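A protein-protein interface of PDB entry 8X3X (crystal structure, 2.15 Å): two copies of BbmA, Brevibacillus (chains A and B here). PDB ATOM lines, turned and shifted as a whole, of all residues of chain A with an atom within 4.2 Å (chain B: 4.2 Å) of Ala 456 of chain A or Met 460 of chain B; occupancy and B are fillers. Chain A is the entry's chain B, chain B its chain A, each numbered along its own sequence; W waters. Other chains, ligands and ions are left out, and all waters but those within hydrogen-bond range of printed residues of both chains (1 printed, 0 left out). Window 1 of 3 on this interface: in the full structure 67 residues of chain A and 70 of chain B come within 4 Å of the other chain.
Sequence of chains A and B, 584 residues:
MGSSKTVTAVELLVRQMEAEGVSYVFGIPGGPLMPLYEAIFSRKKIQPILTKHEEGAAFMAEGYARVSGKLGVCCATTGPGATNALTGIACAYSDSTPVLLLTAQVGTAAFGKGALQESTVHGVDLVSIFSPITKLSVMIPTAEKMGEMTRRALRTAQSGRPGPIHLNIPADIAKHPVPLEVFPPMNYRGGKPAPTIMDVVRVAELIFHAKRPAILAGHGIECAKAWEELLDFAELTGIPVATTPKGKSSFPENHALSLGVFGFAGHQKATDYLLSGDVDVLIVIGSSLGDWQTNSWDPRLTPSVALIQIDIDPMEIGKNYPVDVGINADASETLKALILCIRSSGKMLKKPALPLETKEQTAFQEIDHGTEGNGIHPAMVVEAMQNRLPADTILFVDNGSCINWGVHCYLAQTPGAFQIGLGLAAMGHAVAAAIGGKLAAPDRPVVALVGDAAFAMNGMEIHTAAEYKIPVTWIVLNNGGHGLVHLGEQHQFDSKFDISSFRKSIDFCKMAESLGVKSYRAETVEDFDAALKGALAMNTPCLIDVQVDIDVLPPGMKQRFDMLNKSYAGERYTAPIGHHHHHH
Ala 456 of chain A touches one residue of chain B.
Asn 458 of chain A touches none of the printed residues of chain B.
Of chain A, only Ala 456 (3.3 Å) and Met 511 (3.9 Å) come within 4 Å of Met 460 of chain B.
Printed residues of chain A within 4 Å of His 463 of chain B: Ile 506 (3.6 Å).
Printed residues of chain A within 4 Å of Leu 515 of chain B: Ile 506.
The nearest residue of chain B that does not touch Ala 456 of chain A is Lys 52 of chain B (4.04 Å).
The nearest printed residue of chain B that does not touch Ile 506 of chain A is Met 460 of chain B (4.2 Å).
Water W1 lies within hydrogen-bond range of O of Lys 52 of chain B and O of Ala 453 of chain A.
2 positions are printed for both chains.
N of Lys 52 of chain B is in hydrogen-bond range of OE2 of Glu 461 of chain B (3.0 Å).
The side-chain amino group (NZ) of Lys 52 of chain B sits at hydrogen-bond distance from a ring nitrogen (ND1) of His 463 of chain B, at 2.5 Å.
Of the 9 printed residues of chain A, 4 touch a printed residue of chain B.
Of the 9 printed residues of chain B, 4 touch a printed residue of chain A.
Printed residues of chain B that touch a printed residue of chain A: Lys 52, Met 460, His 463 and Leu 515.
Hydrophobic or aromatic side chains of chain B within 4 Å of the printed part of chain A: Met 460, His 463 and Leu 515.
Among the printed residues, no Asp or Glu carboxylate lies within 4 Å of a Lys or Arg side-chain nitrogen of the other chain.
Among the printed residues, merely in contact across the chains: Met 457 of chain A with Lys 52 of chain B (3.1 Å), Ala 456 of chain A with Met 460 of chain B (3.3 Å), Ile 506 of chain A with His 463 of chain B (3.6 Å), Ile 506 of chain A with Leu 515 of chain B (3.8 Å) and Met 511 of chain A with Met 460 of chain B (3.9 Å).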
ATOM      1  N   ASP A 452     -20.777  20.036 -12.956  1.00  0.00           N
ATOM      2  CA  ASP A 452     -20.510  20.343 -11.549  1.00  0.00           C
ATOM      3  C   ASP A 452     -19.026  20.547 -11.283  1.00  0.00           C
ATOM      4  O   ASP A 452     -18.659  21.428 -10.499  1.00  0.00           O
ATOM      5  CB  ASP A 452     -21.070  19.260 -10.627  1.00  0.00           C
ATOM      6  CG  ASP A 452     -20.571  17.867 -10.959  1.00  0.00           C
ATOM      7  OD1 ASP A 452     -20.611  17.474 -12.146  1.00  0.00           O
ATOM      8  OD2 ASP A 452     -20.174  17.151 -10.007  1.00  0.00           O
ATOM      9  N   ALA A 453     -18.147  19.759 -11.927  1.00  0.00           N
ATOM     10  CA  ALA A 453     -16.714  19.976 -11.712  1.00  0.00           C
ATOM     11  C   ALA A 453     -16.271  21.293 -12.331  1.00  0.00           C
ATOM     12  O   ALA A 453     -15.418  21.990 -11.770  1.00  0.00           O
ATOM     13  CB  ALA A 453     -15.889  18.818 -12.268  1.00  0.00           C
ATOM     14  N   ALA A 454     -16.844  21.655 -13.489  1.00  0.00           N
ATOM     15  CA  ALA A 454     -16.577  22.978 -14.043  1.00  0.00           C
ATOM     16  C   ALA A 454     -17.022  24.067 -13.080  1.00  0.00           C
ATOM     17  O   ALA A 454     -16.321  25.070 -12.901  1.00  0.00           O
ATOM     18  CB  ALA A 454     -17.272  23.151 -15.392  1.00  0.00           C
ATOM     19  N   PHE A 455     -18.184  23.882 -12.444  1.00  0.00           N
ATOM     20  CA  PHE A 455     -18.677  24.899 -11.521  1.00  0.00           C
ATOM     21  C   PHE A 455     -17.778  25.032 -10.298  1.00  0.00           C
ATOM     22  O   PHE A 455     -17.594  26.142  -9.786  1.00  0.00           O
ATOM     23  CB  PHE A 455     -20.120  24.601 -11.105  1.00  0.00           C
ATOM     24  CG  PHE A 455     -20.847  25.804 -10.576  1.00  0.00           C
ATOM     25  CD1 PHE A 455     -21.472  26.689 -11.439  1.00  0.00           C
ATOM     26  CD2 PHE A 455     -20.879  26.067  -9.208  1.00  0.00           C
ATOM     27  CE1 PHE A 455     -22.137  27.809 -10.956  1.00  0.00           C
ATOM     28  CE2 PHE A 455     -21.541  27.186  -8.714  1.00  0.00           C
ATOM     29  CZ  PHE A 455     -22.170  28.058  -9.593  1.00  0.00           C
ATOM     30  N   ALA A 456     -17.193  23.932  -9.821  1.00  0.00           N
ATOM     31  CA  ALA A 456     -16.277  24.057  -8.692  1.00  0.00           C
ATOM     32  C   ALA A 456     -15.035  24.850  -9.068  1.00  0.00           C
ATOM     33  O   ALA A 456     -14.402  25.437  -8.188  1.00  0.00           O
ATOM     34  CB  ALA A 456     -15.878  22.678  -8.153  1.00  0.00           C
ATOM     35  N   MET A 457     -14.703  24.913 -10.360  1.00  0.00           N
ATOM     36  CA  MET A 457     -13.522  25.637 -10.810  1.00  0.00           C
ATOM     37  C   MET A 457     -13.725  27.149 -10.799  1.00  0.00           C
ATOM     38  O   MET A 457     -12.802  27.891 -10.451  1.00  0.00           O
ATOM     39  CB  MET A 457     -13.138  25.189 -12.221  1.00  0.00           C
ATOM     40  CG  MET A 457     -12.233  23.992 -12.240  1.00  0.00           C
ATOM     41  SD  MET A 457     -11.429  23.783 -13.827  1.00  0.00           S
ATOM     42  CE  MET A 457     -11.022  22.039 -13.716  1.00  0.00           C
ATOM     43  N   ASN A 458     -14.911  27.627 -11.218  1.00  0.00           N
ATOM     44  CA  ASN A 458     -15.128  29.059 -11.397  1.00  0.00           C
ATOM     45  C   ASN A 458     -16.500  29.516 -10.922  1.00  0.00           C
ATOM     46  O   ASN A 458     -16.856  30.681 -11.145  1.00  0.00           O
ATOM     47  CB  ASN A 458     -14.940  29.449 -12.873  1.00  0.00           C
ATOM     48  CG  ASN A 458     -13.484  29.344 -13.320  1.00  0.00           C
ATOM     49  OD1 ASN A 458     -13.080  28.348 -13.925  1.00  0.00           O
ATOM     50  ND2 ASN A 458     -12.684  30.367 -13.002  1.00  0.00           N
ATOM     51  N   ILE A 506     -21.274  17.927  -4.388  1.00  0.00           N
ATOM     52  CA  ILE A 506     -21.411  19.277  -3.864  1.00  0.00           C
ATOM     53  C   ILE A 506     -22.882  19.684  -3.876  1.00  0.00           C
ATOM     54  O   ILE A 506     -23.626  19.389  -4.825  1.00  0.00           O
ATOM     55  CB  ILE A 506     -20.535  20.237  -4.690  1.00  0.00           C
ATOM     56  CG1 ILE A 506     -19.065  19.858  -4.518  1.00  0.00           C
ATOM     57  CG2 ILE A 506     -20.787  21.687  -4.303  1.00  0.00           C
ATOM     58  CD1 ILE A 506     -18.103  20.519  -5.511  1.00  0.00           C
ATOM     59  N   MET A 511     -24.447  26.164  -1.774  1.00  0.00           N
ATOM     60  CA  MET A 511     -23.361  27.022  -2.226  1.00  0.00           C
ATOM     61  C   MET A 511     -23.904  28.321  -2.808  1.00  0.00           C
ATOM     62  O   MET A 511     -23.373  29.401  -2.529  1.00  0.00           O
ATOM     63  CB  MET A 511     -22.505  26.294  -3.260  1.00  0.00           C
ATOM     64  CG  MET A 511     -21.305  27.117  -3.741  1.00  0.00           C
ATOM     65  SD  MET A 511     -20.480  26.405  -5.188  1.00  0.00           S
ATOM     66  CE  MET A 511     -19.548  27.808  -5.800  1.00  0.00           C
ATOM     67  N   LYS B  52      -9.833  20.482  -7.151  1.00  0.00           N
ATOM     68  CA  LYS B  52     -10.950  21.170  -7.787  1.00  0.00           C
ATOM     69  C   LYS B  52     -10.496  22.078  -8.926  1.00  0.00           C
ATOM     70  O   LYS B  52     -11.274  22.330  -9.853  1.00  0.00           O
ATOM     71  CB  LYS B  52     -11.739  21.978  -6.739  1.00  0.00           C
ATOM     72  CG  LYS B  52     -12.471  21.105  -5.693  1.00  0.00           C
ATOM     73  CD  LYS B  52     -13.354  20.053  -6.394  1.00  0.00           C
ATOM     74  CE  LYS B  52     -13.068  18.642  -5.847  1.00  0.00           C
ATOM     75  NZ  LYS B  52     -12.954  18.641  -4.363  1.00  0.00           N
ATOM     76  N   ASN B 458      -9.716  30.404  -3.981  1.00  0.00           N
ATOM     77  CA  ASN B 458      -9.315  28.998  -3.995  1.00  0.00           C
ATOM     78  C   ASN B 458      -9.997  28.161  -2.906  1.00  0.00           C
ATOM     79  O   ASN B 458      -9.655  26.983  -2.750  1.00  0.00           O
ATOM     80  CB  ASN B 458      -7.782  28.877  -3.853  1.00  0.00           C
ATOM     81  CG  ASN B 458      -7.023  29.321  -5.121  1.00  0.00           C
ATOM     82  OD1 ASN B 458      -6.596  30.474  -5.231  1.00  0.00           O
ATOM     83  ND2 ASN B 458      -6.859  28.402  -6.077  1.00  0.00           N
ATOM     84  N   GLY B 459     -10.966  28.708  -2.168  1.00  0.00           N
ATOM     85  CA  GLY B 459     -11.599  27.978  -1.071  1.00  0.00           C
ATOM     86  C   GLY B 459     -12.370  26.730  -1.473  1.00  0.00           C
ATOM     87  O   GLY B 459     -12.677  25.899  -0.610  1.00  0.00           O
ATOM     88  N   MET B 460     -12.685  26.567  -2.761  1.00  0.00           N
ATOM     89  CA  MET B 460     -13.372  25.347  -3.185  1.00  0.00           C
ATOM     90  C   MET B 460     -12.551  24.103  -2.865  1.00  0.00           C
ATOM     91  O   MET B 460     -13.123  23.023  -2.674  1.00  0.00           O
ATOM     92  CB  MET B 460     -13.696  25.397  -4.685  1.00  0.00           C
ATOM     93  CG  MET B 460     -14.774  26.408  -5.047  1.00  0.00           C
ATOM     94  SD  MET B 460     -16.420  26.006  -4.374  1.00  0.00           S
ATOM     95  CE  MET B 460     -16.767  24.446  -5.168  1.00  0.00           C
ATOM     96  N   GLU B 461     -11.212  24.237  -2.775  1.00  0.00           N
ATOM     97  CA  GLU B 461     -10.346  23.098  -2.456  1.00  0.00           C
ATOM     98  C   GLU B 461     -10.659  22.457  -1.108  1.00  0.00           C
ATOM     99  O   GLU B 461     -10.198  21.337  -0.855  1.00  0.00           O
ATOM    100  CB  GLU B 461      -8.864  23.507  -2.458  1.00  0.00           C
ATOM    101  CG  GLU B 461      -8.297  23.870  -3.834  1.00  0.00           C
ATOM    102  CD  GLU B 461      -8.516  22.789  -4.916  1.00  0.00           C
ATOM    103  OE1 GLU B 461      -8.378  23.145  -6.107  1.00  0.00           O
ATOM    104  OE2 GLU B 461      -8.834  21.607  -4.596  1.00  0.00           O
ATOM    105  N   ILE B 462     -11.408  23.124  -0.221  1.00  0.00           N
ATOM    106  CA  ILE B 462     -11.733  22.457   1.046  1.00  0.00           C
ATOM    107  C   ILE B 462     -12.570  21.214   0.769  1.00  0.00           C
ATOM    108  O   ILE B 462     -12.618  20.289   1.593  1.00  0.00           O
ATOM    109  CB  ILE B 462     -12.451  23.383   2.077  1.00  0.00           C
ATOM    110  CG1 ILE B 462     -13.894  23.710   1.664  1.00  0.00           C
ATOM    111  CG2 ILE B 462     -11.639  24.642   2.358  1.00  0.00           C
ATOM    112  CD1 ILE B 462     -14.654  24.474   2.743  1.00  0.00           C
ATOM    113  N   HIS B 463     -13.222  21.160  -0.391  1.00  0.00           N
ATOM    114  CA  HIS B 463     -13.932  19.943  -0.769  1.00  0.00           C
ATOM    115  C   HIS B 463     -12.951  18.795  -0.986  1.00  0.00           C
ATOM    116  O   HIS B 463     -13.235  17.647  -0.626  1.00  0.00           O
ATOM    117  CB  HIS B 463     -14.768  20.201  -2.020  1.00  0.00           C
ATOM    118  CG  HIS B 463     -15.609  19.040  -2.437  1.00  0.00           C
ATOM    119  ND1 HIS B 463     -15.304  18.260  -3.530  1.00  0.00           N
ATOM    120  CD2 HIS B 463     -16.745  18.525  -1.909  1.00  0.00           C
ATOM    121  CE1 HIS B 463     -16.222  17.317  -3.664  1.00  0.00           C
ATOM    122  NE2 HIS B 463     -17.108  17.457  -2.695  1.00  0.00           N
ATOM    123  N   MET B 511     -21.134  27.997   2.835  1.00  0.00           N
ATOM    124  CA  MET B 511     -20.270  27.444   1.801  1.00  0.00           C
ATOM    125  C   MET B 511     -19.575  26.173   2.275  1.00  0.00           C
ATOM    126  O   MET B 511     -19.541  25.173   1.551  1.00  0.00           O
ATOM    127  CB  MET B 511     -19.237  28.462   1.357  1.00  0.00           C
ATOM    128  CG  MET B 511     -18.456  27.932   0.160  1.00  0.00           C
ATOM    129  SD  MET B 511     -17.007  28.925  -0.167  1.00  0.00           S
ATOM    130  CE  MET B 511     -16.314  28.005  -1.571  1.00  0.00           C
ATOM    131  N   LEU B 515     -19.896  22.125   0.879  1.00  0.00           N
ATOM    132  CA  LEU B 515     -18.787  21.272   0.478  1.00  0.00           C
ATOM    133  C   LEU B 515     -18.535  20.130   1.465  1.00  0.00           C
ATOM    134  O   LEU B 515     -17.518  19.444   1.348  1.00  0.00           O
ATOM    135  CB  LEU B 515     -17.518  22.123   0.302  1.00  0.00           C
ATOM    136  CG  LEU B 515     -17.691  23.283  -0.699  1.00  0.00           C
ATOM    137  CD1 LEU B 515     -16.549  24.297  -0.647  1.00  0.00           C
ATOM    138  CD2 LEU B 515     -17.843  22.749  -2.124  1.00  0.00           C
HETATM  139  O   HOH W   1     -13.404  20.863 -10.420  1.00  0.00           O
